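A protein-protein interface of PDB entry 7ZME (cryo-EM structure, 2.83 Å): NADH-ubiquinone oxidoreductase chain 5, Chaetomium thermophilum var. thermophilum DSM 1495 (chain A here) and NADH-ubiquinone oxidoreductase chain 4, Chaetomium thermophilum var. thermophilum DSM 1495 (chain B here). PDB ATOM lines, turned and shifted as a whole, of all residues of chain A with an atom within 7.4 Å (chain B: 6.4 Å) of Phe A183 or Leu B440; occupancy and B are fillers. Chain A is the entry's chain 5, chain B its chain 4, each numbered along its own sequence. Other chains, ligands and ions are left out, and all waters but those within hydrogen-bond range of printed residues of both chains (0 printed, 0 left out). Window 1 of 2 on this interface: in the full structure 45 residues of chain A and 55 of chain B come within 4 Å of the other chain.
Among the printed residues, merely in contact across the chains: Phe A183 with Phe B437, Phe A70 with Tyr B441, Trp A187 with Tyr B441, Phe A183 with Leu B444, Trp A187 with Glu B445, Phe A183 with Tyr B441, Leu A186 with Tyr B441, Phe A183 with Leu B440, Leu A134 with Phe B437, Leu A186 with Phe B437, Val A180 with Ser B455, Phe A183 with Ser B455 and Trp A187 with Leu B444.
O of Gly B451 sits at hydrogen-bond distance from OG of Ser B455 (2.7 Å). The side-chain hydroxyl of Tyr B441 lies within hydrogen-bond range of the side-chain carboxylate of Glu B445 (3.2 Å).
Printed residues of chain B that touch a printed residue of chain A: Phe B437, Leu B440, Tyr B441, Leu B444, Glu B445 and Ser B455. Hydrophobic or aromatic side chains of chain B that line the printed part of chain A: Phe B437, Leu B440, Tyr B441 and Leu B444. Of the 18 printed residues of chain A, 7 touch a printed residue of chain B. Printed residues of chain A that touch a printed residue of chain B: Phe A70, Leu A134, Cys A176, Val A180, Phe A183, Leu A186 and Trp A187. Hydrophobic or aromatic side chains of chain A that line the printed part of chain B: Phe A70, Leu A134, Val A180, Phe A183, Leu A186 and Trp A187. Among the printed residues, no Asp or Glu carboxylate lies within 4 Å of a Lys or Arg side-chain nitrogen of the other chain.
O of Ser B455 sits at hydrogen-bond distance from SG of Cys A176, 3.2 Å away.
Printed residues of chain B within 4 Å of Phe A183: Phe B437 (3.2 Å), Leu B440 (3.5 Å), Tyr B441 (3.5 Å), Leu B444 (3.4 Å) and Ser B455 (3.98 Å). Of the printed residues of chain A, Leu B440 touches Phe A183 (3.5 Å). Of the printed residues of chain B, Cys A176 touches Ser B455. Of the printed residues of chain A, Leu B444 touches Phe A183 (3.4 Å) and Trp A187 (3.99 Å). Printed residues of chain B within 4 Å of Leu A186: Phe B437 (3.9 Å) and Tyr B441 (3.5 Å). Of the printed residues of chain B, Phe A70 touches Tyr B441. The nearest residue of chain B that does not touch Phe A183 is Glu B436 (5.0 Å). The nearest residue of chain A that does not touch Leu B440 is Thr A179 (5.3 Å). The nearest printed residue of chain B that does not touch Cys A176 is Ile B458 (4.3 Å).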
ATOM      1  N   PHE A  70      18.091 -29.869   4.021  1.00  0.00           N
ATOM      2  CA  PHE A  70      18.026 -29.910   5.474  1.00  0.00           C
ATOM      3  C   PHE A  70      16.606 -29.610   5.926  1.00  0.00           C
ATOM      4  O   PHE A  70      16.041 -28.571   5.573  1.00  0.00           O
ATOM      5  CB  PHE A  70      19.009 -28.912   6.083  1.00  0.00           C
ATOM      6  CG  PHE A  70      20.403 -29.007   5.525  1.00  0.00           C
ATOM      7  CD1 PHE A  70      20.864 -30.183   4.955  1.00  0.00           C
ATOM      8  CD2 PHE A  70      21.256 -27.918   5.572  1.00  0.00           C
ATOM      9  CE1 PHE A  70      22.137 -30.267   4.440  1.00  0.00           C
ATOM     10  CE2 PHE A  70      22.532 -28.003   5.060  1.00  0.00           C
ATOM     11  CZ  PHE A  70      22.970 -29.176   4.496  1.00  0.00           C
ATOM     12  N   LEU A 134      20.478 -30.054  16.185  1.00  0.00           N
ATOM     13  CA  LEU A 134      20.259 -28.612  16.155  1.00  0.00           C
ATOM     14  C   LEU A 134      19.215 -28.170  17.168  1.00  0.00           C
ATOM     15  O   LEU A 134      19.376 -27.126  17.808  1.00  0.00           O
ATOM     16  CB  LEU A 134      19.860 -28.169  14.748  1.00  0.00           C
ATOM     17  CG  LEU A 134      20.203 -26.719  14.411  1.00  0.00           C
ATOM     18  CD1 LEU A 134      21.638 -26.418  14.785  1.00  0.00           C
ATOM     19  CD2 LEU A 134      19.974 -26.459  12.946  1.00  0.00           C
ATOM     20  N   CYS A 176      31.595 -23.611  19.338  1.00  0.00           N
ATOM     21  CA  CYS A 176      32.232 -23.408  18.024  1.00  0.00           C
ATOM     22  C   CYS A 176      32.526 -24.778  17.425  1.00  0.00           C
ATOM     23  O   CYS A 176      32.100 -25.003  16.312  1.00  0.00           O
ATOM     24  CB  CYS A 176      33.482 -22.542  18.155  1.00  0.00           C
ATOM     25  SG  CYS A 176      34.469 -22.419  16.645  1.00  0.00           S
ATOM     26  N   PHE A 177      33.225 -25.651  18.147  1.00  0.00           N
ATOM     27  CA  PHE A 177      33.483 -26.997  17.654  1.00  0.00           C
ATOM     28  C   PHE A 177      32.201 -27.810  17.549  1.00  0.00           C
ATOM     29  O   PHE A 177      32.061 -28.622  16.630  1.00  0.00           O
ATOM     30  CB  PHE A 177      34.494 -27.701  18.555  1.00  0.00           C
ATOM     31  CG  PHE A 177      35.845 -27.054  18.562  1.00  0.00           C
ATOM     32  CD1 PHE A 177      36.069 -25.889  19.274  1.00  0.00           C
ATOM     33  CD2 PHE A 177      36.895 -27.613  17.857  1.00  0.00           C
ATOM     34  CE1 PHE A 177      37.306 -25.295  19.279  1.00  0.00           C
ATOM     35  CE2 PHE A 177      38.138 -27.020  17.860  1.00  0.00           C
ATOM     36  CZ  PHE A 177      38.343 -25.861  18.573  1.00  0.00           C
ATOM     37  N   LEU A 178      31.258 -27.609  18.469  1.00  0.00           N
ATOM     38  CA  LEU A 178      29.970 -28.275  18.338  1.00  0.00           C
ATOM     39  C   LEU A 178      29.247 -27.821  17.076  1.00  0.00           C
ATOM     40  O   LEU A 178      28.675 -28.643  16.352  1.00  0.00           O
ATOM     41  CB  LEU A 178      29.108 -28.015  19.573  1.00  0.00           C
ATOM     42  CG  LEU A 178      27.781 -28.779  19.598  1.00  0.00           C
ATOM     43  CD1 LEU A 178      27.986 -30.230  19.207  1.00  0.00           C
ATOM     44  CD2 LEU A 178      27.124 -28.685  20.951  1.00  0.00           C
ATOM     45  N   THR A 179      29.264 -26.516  16.797  1.00  0.00           N
ATOM     46  CA  THR A 179      28.621 -26.005  15.592  1.00  0.00           C
ATOM     47  C   THR A 179      29.324 -26.504  14.337  1.00  0.00           C
ATOM     48  O   THR A 179      28.669 -26.841  13.344  1.00  0.00           O
ATOM     49  CB  THR A 179      28.589 -24.475  15.622  1.00  0.00           C
ATOM     50  OG1 THR A 179      27.739 -24.037  16.687  1.00  0.00           O
ATOM     51  CG2 THR A 179      28.070 -23.917  14.308  1.00  0.00           C
ATOM     52  N   VAL A 180      30.655 -26.562  14.364  1.00  0.00           N
ATOM     53  CA  VAL A 180      31.400 -27.076  13.219  1.00  0.00           C
ATOM     54  C   VAL A 180      31.149 -28.568  13.043  1.00  0.00           C
ATOM     55  O   VAL A 180      31.064 -29.069  11.916  1.00  0.00           O
ATOM     56  CB  VAL A 180      32.898 -26.752  13.376  1.00  0.00           C
ATOM     57  CG1 VAL A 180      33.746 -27.659  12.511  1.00  0.00           C
ATOM     58  CG2 VAL A 180      33.155 -25.301  13.023  1.00  0.00           C
ATOM     59  N   GLY A 181      31.019 -29.300  14.149  1.00  0.00           N
ATOM     60  CA  GLY A 181      30.746 -30.725  14.050  1.00  0.00           C
ATOM     61  C   GLY A 181      29.404 -31.022  13.414  1.00  0.00           C
ATOM     62  O   GLY A 181      29.270 -31.972  12.641  1.00  0.00           O
ATOM     63  N   MET A 182      28.390 -30.217  13.737  1.00  0.00           N
ATOM     64  CA  MET A 182      27.105 -30.341  13.060  1.00  0.00           C
ATOM     65  C   MET A 182      27.211 -29.956  11.593  1.00  0.00           C
ATOM     66  O   MET A 182      26.504 -30.525  10.755  1.00  0.00           O
ATOM     67  CB  MET A 182      26.059 -29.486  13.769  1.00  0.00           C
ATOM     68  CG  MET A 182      25.925 -29.789  15.247  1.00  0.00           C
ATOM     69  SD  MET A 182      24.470 -29.042  15.996  1.00  0.00           S
ATOM     70  CE  MET A 182      25.127 -27.466  16.529  1.00  0.00           C
ATOM     71  N   PHE A 183      28.082 -29.000  11.263  1.00  0.00           N
ATOM     72  CA  PHE A 183      28.331 -28.678   9.861  1.00  0.00           C
ATOM     73  C   PHE A 183      28.893 -29.880   9.119  1.00  0.00           C
ATOM     74  O   PHE A 183      28.516 -30.145   7.973  1.00  0.00           O
ATOM     75  CB  PHE A 183      29.299 -27.504   9.748  1.00  0.00           C
ATOM     76  CG  PHE A 183      28.705 -26.176  10.094  1.00  0.00           C
ATOM     77  CD1 PHE A 183      27.343 -25.975  10.065  1.00  0.00           C
ATOM     78  CD2 PHE A 183      29.525 -25.118  10.441  1.00  0.00           C
ATOM     79  CE1 PHE A 183      26.812 -24.745  10.379  1.00  0.00           C
ATOM     80  CE2 PHE A 183      28.996 -23.893  10.764  1.00  0.00           C
ATOM     81  CZ  PHE A 183      27.638 -23.706  10.734  1.00  0.00           C
ATOM     82  N   ALA A 184      29.812 -30.614   9.755  1.00  0.00           N
ATOM     83  CA  ALA A 184      30.352 -31.830   9.160  1.00  0.00           C
ATOM     84  C   ALA A 184      29.288 -32.904   9.007  1.00  0.00           C
ATOM     85  O   ALA A 184      29.339 -33.691   8.059  1.00  0.00           O
ATOM     86  CB  ALA A 184      31.513 -32.354  10.001  1.00  0.00           C
ATOM     87  N   ILE A 185      28.329 -32.963   9.933  1.00  0.00           N
ATOM     88  CA  ILE A 185      27.247 -33.936   9.825  1.00  0.00           C
ATOM     89  C   ILE A 185      26.314 -33.573   8.679  1.00  0.00           C
ATOM     90  O   ILE A 185      25.893 -34.440   7.905  1.00  0.00           O
ATOM     91  CB  ILE A 185      26.496 -34.036  11.166  1.00  0.00           C
ATOM     92  CG1 ILE A 185      27.360 -34.736  12.212  1.00  0.00           C
ATOM     93  CG2 ILE A 185      25.178 -34.773  11.001  1.00  0.00           C
ATOM     94  CD1 ILE A 185      26.749 -34.740  13.585  1.00  0.00           C
ATOM     95  N   LEU A 186      25.973 -32.288   8.548  1.00  0.00           N
ATOM     96  CA  LEU A 186      25.124 -31.848   7.444  1.00  0.00           C
ATOM     97  C   LEU A 186      25.812 -32.052   6.104  1.00  0.00           C
ATOM     98  O   LEU A 186      25.167 -32.415   5.116  1.00  0.00           O
ATOM     99  CB  LEU A 186      24.747 -30.377   7.615  1.00  0.00           C
ATOM    100  CG  LEU A 186      23.584 -30.014   8.529  1.00  0.00           C
ATOM    101  CD1 LEU A 186      23.374 -28.510   8.521  1.00  0.00           C
ATOM    102  CD2 LEU A 186      22.319 -30.743   8.122  1.00  0.00           C
ATOM    103  N   TRP A 187      27.120 -31.799   6.047  1.00  0.00           N
ATOM    104  CA  TRP A 187      27.855 -31.975   4.801  1.00  0.00           C
ATOM    105  C   TRP A 187      27.808 -33.423   4.338  1.00  0.00           C
ATOM    106  O   TRP A 187      27.478 -33.707   3.183  1.00  0.00           O
ATOM    107  CB  TRP A 187      29.302 -31.515   4.975  1.00  0.00           C
ATOM    108  CG  TRP A 187      30.032 -31.296   3.681  1.00  0.00           C
ATOM    109  CD1 TRP A 187      29.593 -31.607   2.430  1.00  0.00           C
ATOM    110  CD2 TRP A 187      31.335 -30.732   3.518  1.00  0.00           C
ATOM    111  NE1 TRP A 187      30.537 -31.266   1.499  1.00  0.00           N
ATOM    112  CE2 TRP A 187      31.619 -30.729   2.143  1.00  0.00           C
ATOM    113  CE3 TRP A 187      32.289 -30.228   4.403  1.00  0.00           C
ATOM    114  CZ2 TRP A 187      32.815 -30.239   1.631  1.00  0.00           C
ATOM    115  CZ3 TRP A 187      33.474 -29.745   3.892  1.00  0.00           C
ATOM    116  CH2 TRP A 187      33.727 -29.753   2.521  1.00  0.00           C
ATOM    117  N   SER A 188      28.115 -34.356   5.233  1.00  0.00           N
ATOM    118  CA  SER A 188      28.266 -35.748   4.844  1.00  0.00           C
ATOM    119  C   SER A 188      26.963 -36.540   4.854  1.00  0.00           C
ATOM    120  O   SER A 188      26.938 -37.650   4.316  1.00  0.00           O
ATOM    121  CB  SER A 188      29.291 -36.437   5.747  1.00  0.00           C
ATOM    122  OG  SER A 188      28.882 -36.414   7.096  1.00  0.00           O
ATOM    123  N   LEU A 189      25.887 -36.021   5.440  1.00  0.00           N
ATOM    124  CA  LEU A 189      24.639 -36.772   5.496  1.00  0.00           C
ATOM    125  C   LEU A 189      23.430 -36.037   4.946  1.00  0.00           C
ATOM    126  O   LEU A 189      22.411 -36.687   4.687  1.00  0.00           O
ATOM    127  CB  LEU A 189      24.320 -37.206   6.935  1.00  0.00           C
ATOM    128  CG  LEU A 189      24.983 -38.473   7.489  1.00  0.00           C
ATOM    129  CD1 LEU A 189      24.542 -39.698   6.705  1.00  0.00           C
ATOM    130  CD2 LEU A 189      26.492 -38.373   7.554  1.00  0.00           C
ATOM    131  N   LEU A 192      20.703 -33.897  10.089  1.00  0.00           N
ATOM    132  CA  LEU A 192      21.275 -34.177  11.398  1.00  0.00           C
ATOM    133  C   LEU A 192      20.244 -34.699  12.396  1.00  0.00           C
ATOM    134  O   LEU A 192      20.455 -34.582  13.607  1.00  0.00           O
ATOM    135  CB  LEU A 192      22.022 -32.928  11.893  1.00  0.00           C
ATOM    136  CG  LEU A 192      21.313 -31.594  12.109  1.00  0.00           C
ATOM    137  CD1 LEU A 192      20.626 -31.494  13.428  1.00  0.00           C
ATOM    138  CD2 LEU A 192      22.330 -30.474  11.966  1.00  0.00           C
ATOM    139  N   ILE A 212      33.945 -35.671  12.885  1.00  0.00           N
ATOM    140  CA  ILE A 212      32.711 -35.368  13.605  1.00  0.00           C
ATOM    141  C   ILE A 212      32.881 -35.639  15.093  1.00  0.00           C
ATOM    142  O   ILE A 212      32.473 -34.832  15.937  1.00  0.00           O
ATOM    143  CB  ILE A 212      31.539 -36.172  13.014  1.00  0.00           C
ATOM    144  CG1 ILE A 212      31.143 -35.603  11.652  1.00  0.00           C
ATOM    145  CG2 ILE A 212      30.355 -36.175  13.972  1.00  0.00           C
ATOM    146  CD1 ILE A 212      30.375 -36.572  10.786  1.00  0.00           C
ATOM    147  N   ILE B 353      30.184 -12.138   7.277  1.00  0.00           N
ATOM    148  CA  ILE B 353      29.689 -13.507   7.349  1.00  0.00           C
ATOM    149  C   ILE B 353      28.717 -13.795   6.214  1.00  0.00           C
ATOM    150  O   ILE B 353      28.800 -14.845   5.568  1.00  0.00           O
ATOM    151  CB  ILE B 353      29.060 -13.781   8.727  1.00  0.00           C
ATOM    152  CG1 ILE B 353      30.105 -13.621   9.826  1.00  0.00           C
ATOM    153  CG2 ILE B 353      28.483 -15.186   8.780  1.00  0.00           C
ATOM    154  CD1 ILE B 353      31.066 -14.776   9.914  1.00  0.00           C
ATOM    155  N   MET B 356      30.534 -13.919   2.838  1.00  0.00           N
ATOM    156  CA  MET B 356      31.102 -15.227   2.543  1.00  0.00           C
ATOM    157  C   MET B 356      30.020 -16.236   2.188  1.00  0.00           C
ATOM    158  O   MET B 356      30.268 -17.153   1.398  1.00  0.00           O
ATOM    159  CB  MET B 356      31.927 -15.724   3.726  1.00  0.00           C
ATOM    160  CG  MET B 356      33.269 -15.042   3.880  1.00  0.00           C
ATOM    161  SD  MET B 356      33.997 -15.353   5.494  1.00  0.00           S
ATOM    162  CE  MET B 356      35.439 -16.303   5.025  1.00  0.00           C
ATOM    163  N   GLY B 357      28.824 -16.088   2.759  1.00  0.00           N
ATOM    164  CA  GLY B 357      27.745 -17.003   2.442  1.00  0.00           C
ATOM    165  C   GLY B 357      27.137 -16.773   1.075  1.00  0.00           C
ATOM    166  O   GLY B 357      26.593 -17.700   0.472  1.00  0.00           O
ATOM    167  N   GLY B 365      23.918 -21.583   1.940  1.00  0.00           N
ATOM    168  CA  GLY B 365      24.678 -20.384   2.243  1.00  0.00           C
ATOM    169  C   GLY B 365      24.038 -19.135   1.678  1.00  0.00           C
ATOM    170  O   GLY B 365      23.997 -18.095   2.339  1.00  0.00           O
ATOM    171  N   GLY B 435      20.523 -17.385  10.154  1.00  0.00           N
ATOM    172  CA  GLY B 435      21.340 -16.830   9.087  1.00  0.00           C
ATOM    173  C   GLY B 435      22.820 -17.081   9.302  1.00  0.00           C
ATOM    174  O   GLY B 435      23.550 -17.418   8.367  1.00  0.00           O
ATOM    175  N   GLU B 436      23.281 -16.908  10.541  1.00  0.00           N
ATOM    176  CA  GLU B 436      24.664 -17.216  10.887  1.00  0.00           C
ATOM    177  C   GLU B 436      24.977 -18.680  10.603  1.00  0.00           C
ATOM    178  O   GLU B 436      25.988 -19.004   9.975  1.00  0.00           O
ATOM    179  CB  GLU B 436      24.889 -16.891  12.365  1.00  0.00           C
ATOM    180  CG  GLU B 436      26.291 -17.103  12.902  1.00  0.00           C
ATOM    181  CD  GLU B 436      27.309 -16.175  12.284  1.00  0.00           C
ATOM    182  OE1 GLU B 436      26.917 -15.079  11.834  1.00  0.00           O
ATOM    183  OE2 GLU B 436      28.503 -16.532  12.266  1.00  0.00           O
ATOM    184  N   PHE B 437      24.095 -19.579  11.048  1.00  0.00           N
ATOM    185  CA  PHE B 437      24.347 -21.012  10.942  1.00  0.00           C
ATOM    186  C   PHE B 437      24.355 -21.476   9.491  1.00  0.00           C
ATOM    187  O   PHE B 437      25.204 -22.281   9.093  1.00  0.00           O
ATOM    188  CB  PHE B 437      23.296 -21.778  11.748  1.00  0.00           C
ATOM    189  CG  PHE B 437      23.469 -23.267  11.720  1.00  0.00           C
ATOM    190  CD1 PHE B 437      24.311 -23.895  12.617  1.00  0.00           C
ATOM    191  CD2 PHE B 437      22.784 -24.040  10.798  1.00  0.00           C
ATOM    192  CE1 PHE B 437      24.469 -25.259  12.597  1.00  0.00           C
ATOM    193  CE2 PHE B 437      22.943 -25.402  10.772  1.00  0.00           C
ATOM    194  CZ  PHE B 437      23.788 -26.013  11.675  1.00  0.00           C
ATOM    195  N   MET B 438      23.414 -20.984   8.683  1.00  0.00           N
ATOM    196  CA  MET B 438      23.292 -21.475   7.314  1.00  0.00           C
ATOM    197  C   MET B 438      24.384 -20.917   6.409  1.00  0.00           C
ATOM    198  O   MET B 438      24.889 -21.629   5.534  1.00  0.00           O
ATOM    199  CB  MET B 438      21.912 -21.149   6.753  1.00  0.00           C
ATOM    200  CG  MET B 438      20.770 -21.880   7.422  1.00  0.00           C
ATOM    201  SD  MET B 438      19.176 -21.372   6.755  1.00  0.00           S
ATOM    202  CE  MET B 438      19.243 -22.098   5.128  1.00  0.00           C
ATOM    203  N   SER B 439      24.760 -19.652   6.589  1.00  0.00           N
ATOM    204  CA  SER B 439      25.798 -19.086   5.735  1.00  0.00           C
ATOM    205  C   SER B 439      27.182 -19.566   6.156  1.00  0.00           C
ATOM    206  O   SER B 439      28.127 -19.521   5.363  1.00  0.00           O
ATOM    207  CB  SER B 439      25.719 -17.557   5.735  1.00  0.00           C
ATOM    208  OG  SER B 439      25.676 -17.035   7.046  1.00  0.00           O
ATOM    209  N   LEU B 440      27.321 -20.029   7.397  1.00  0.00           N
ATOM    210  CA  LEU B 440      28.581 -20.628   7.817  1.00  0.00           C
ATOM    211  C   LEU B 440      28.740 -22.040   7.273  1.00  0.00           C
ATOM    212  O   LEU B 440      29.856 -22.448   6.939  1.00  0.00           O
ATOM    213  CB  LEU B 440      28.684 -20.636   9.338  1.00  0.00           C
ATOM    214  CG  LEU B 440      29.199 -19.358   9.994  1.00  0.00           C
ATOM    215  CD1 LEU B 440      29.298 -19.567  11.478  1.00  0.00           C
ATOM    216  CD2 LEU B 440      30.533 -18.944   9.420  1.00  0.00           C
ATOM    217  N   TYR B 441      27.648 -22.802   7.190  1.00  0.00           N
ATOM    218  CA  TYR B 441      27.718 -24.111   6.558  1.00  0.00           C
ATOM    219  C   TYR B 441      28.083 -23.996   5.083  1.00  0.00           C
ATOM    220  O   TYR B 441      28.899 -24.777   4.582  1.00  0.00           O
ATOM    221  CB  TYR B 441      26.391 -24.854   6.715  1.00  0.00           C
ATOM    222  CG  TYR B 441      26.306 -26.087   5.845  1.00  0.00           C
ATOM    223  CD1 TYR B 441      26.863 -27.286   6.254  1.00  0.00           C
ATOM    224  CD2 TYR B 441      25.680 -26.046   4.608  1.00  0.00           C
ATOM    225  CE1 TYR B 441      26.797 -28.404   5.458  1.00  0.00           C
ATOM    226  CE2 TYR B 441      25.616 -27.158   3.808  1.00  0.00           C
ATOM    227  CZ  TYR B 441      26.174 -28.334   4.237  1.00  0.00           C
ATOM    228  OH  TYR B 441      26.107 -29.452   3.445  1.00  0.00           O
ATOM    229  N   GLY B 442      27.480 -23.044   4.372  1.00  0.00           N
ATOM    230  CA  GLY B 442      27.833 -22.849   2.978  1.00  0.00           C
ATOM    231  C   GLY B 442      29.271 -22.404   2.806  1.00  0.00           C
ATOM    232  O   GLY B 442      29.978 -22.884   1.917  1.00  0.00           O
ATOM    233  N   THR B 443      29.721 -21.478   3.652  1.00  0.00           N
ATOM    234  CA  THR B 443      31.114 -21.050   3.614  1.00  0.00           C
ATOM    235  C   THR B 443      32.048 -22.219   3.883  1.00  0.00           C
ATOM    236  O   THR B 443      33.064 -22.380   3.201  1.00  0.00           O
ATOM    237  CB  THR B 443      31.346 -19.932   4.633  1.00  0.00           C
ATOM    238  OG1 THR B 443      30.294 -18.967   4.532  1.00  0.00           O
ATOM    239  CG2 THR B 443      32.677 -19.248   4.397  1.00  0.00           C
ATOM    240  N   LEU B 444      31.714 -23.048   4.872  1.00  0.00           N
ATOM    241  CA  LEU B 444      32.548 -24.197   5.205  1.00  0.00           C
ATOM    242  C   LEU B 444      32.558 -25.217   4.073  1.00  0.00           C
ATOM    243  O   LEU B 444      33.609 -25.757   3.717  1.00  0.00           O
ATOM    244  CB  LEU B 444      32.047 -24.842   6.494  1.00  0.00           C
ATOM    245  CG  LEU B 444      32.866 -26.021   7.008  1.00  0.00           C
ATOM    246  CD1 LEU B 444      34.256 -25.561   7.352  1.00  0.00           C
ATOM    247  CD2 LEU B 444      32.221 -26.654   8.201  1.00  0.00           C
ATOM    248  N   GLU B 445      31.389 -25.504   3.504  1.00  0.00           N
ATOM    249  CA  GLU B 445      31.308 -26.504   2.448  1.00  0.00           C
ATOM    250  C   GLU B 445      31.991 -26.028   1.171  1.00  0.00           C
ATOM    251  O   GLU B 445      32.429 -26.849   0.358  1.00  0.00           O
ATOM    252  CB  GLU B 445      29.839 -26.862   2.207  1.00  0.00           C
ATOM    253  CG  GLU B 445      29.554 -27.700   0.978  1.00  0.00           C
ATOM    254  CD  GLU B 445      28.084 -28.034   0.840  1.00  0.00           C
ATOM    255  OE1 GLU B 445      27.749 -29.233   0.750  1.00  0.00           O
ATOM    256  OE2 GLU B 445      27.260 -27.103   0.831  1.00  0.00           O
ATOM    257  N   ALA B 450      38.434 -21.526   5.224  1.00  0.00           N
ATOM    258  CA  ALA B 450      37.848 -20.196   5.345  1.00  0.00           C
ATOM    259  C   ALA B 450      36.587 -20.231   6.199  1.00  0.00           C
ATOM    260  O   ALA B 450      36.349 -19.321   7.000  1.00  0.00           O
ATOM    261  CB  ALA B 450      37.547 -19.628   3.961  1.00  0.00           C
ATOM    262  N   GLY B 451      35.767 -21.268   6.034  1.00  0.00           N
ATOM    263  CA  GLY B 451      34.611 -21.435   6.893  1.00  0.00           C
ATOM    264  C   GLY B 451      34.980 -21.692   8.338  1.00  0.00           C
ATOM    265  O   GLY B 451      34.276 -21.246   9.245  1.00  0.00           O
ATOM    266  N   ALA B 454      36.062 -18.295   9.601  1.00  0.00           N
ATOM    267  CA  ALA B 454      34.824 -17.545   9.753  1.00  0.00           C
ATOM    268  C   ALA B 454      33.983 -18.049  10.916  1.00  0.00           C
ATOM    269  O   ALA B 454      33.230 -17.270  11.506  1.00  0.00           O
ATOM    270  CB  ALA B 454      34.010 -17.601   8.461  1.00  0.00           C
ATOM    271  N   SER B 455      34.097 -19.330  11.265  1.00  0.00           N
ATOM    272  CA  SER B 455      33.303 -19.915  12.337  1.00  0.00           C
ATOM    273  C   SER B 455      33.848 -19.600  13.719  1.00  0.00           C
ATOM    274  O   SER B 455      33.366 -20.164  14.705  1.00  0.00           O
ATOM    275  CB  SER B 455      33.201 -21.429  12.154  1.00  0.00           C
ATOM    276  OG  SER B 455      32.328 -21.749  11.084  1.00  0.00           O
ATOM    277  N   THR B 456      34.837 -18.722  13.818  1.00  0.00           N
ATOM    278  CA  THR B 456      35.292 -18.225  15.106  1.00  0.00           C
ATOM    279  C   THR B 456      34.483 -17.028  15.574  1.00  0.00           C
ATOM    280  O   THR B 456      34.757 -16.496  16.653  1.00  0.00           O
ATOM    281  CB  THR B 456      36.777 -17.861  15.038  1.00  0.00           C
ATOM    282  OG1 THR B 456      36.982 -16.857  14.037  1.00  0.00           O
ATOM    283  CG2 THR B 456      37.601 -19.084  14.692  1.00  0.00           C
ATOM    284  N   SER B 457      33.495 -16.592  14.789  1.00  0.00           N
ATOM    285  CA  SER B 457      32.616 -15.515  15.222  1.00  0.00           C
ATOM    286  C   SER B 457      31.621 -15.979  16.272  1.00  0.00           C
ATOM    287  O   SER B 457      31.093 -15.147  17.012  1.00  0.00           O
ATOM    288  CB  SER B 457      31.875 -14.918  14.027  1.00  0.00           C
ATOM    289  OG  SER B 457      30.978 -15.851  13.451  1.00  0.00           O
ATOM    290  N   ILE B 458      31.356 -17.283  16.362  1.00  0.00           N
ATOM    291  CA  ILE B 458      30.566 -17.796  17.478  1.00  0.00           C
ATOM    292  C   ILE B 458      31.236 -17.444  18.796  1.00  0.00           C
ATOM    293  O   ILE B 458      30.571 -17.070  19.770  1.00  0.00           O
ATOM    294  CB  ILE B 458      30.334 -19.313  17.336  1.00  0.00           C
ATOM    295  CG1 ILE B 458      29.514 -19.628  16.080  1.00  0.00           C
ATOM    296  CG2 ILE B 458      29.659 -19.885  18.569  1.00  0.00           C
ATOM    297  CD1 ILE B 458      30.317 -19.841  14.834  1.00  0.00           C
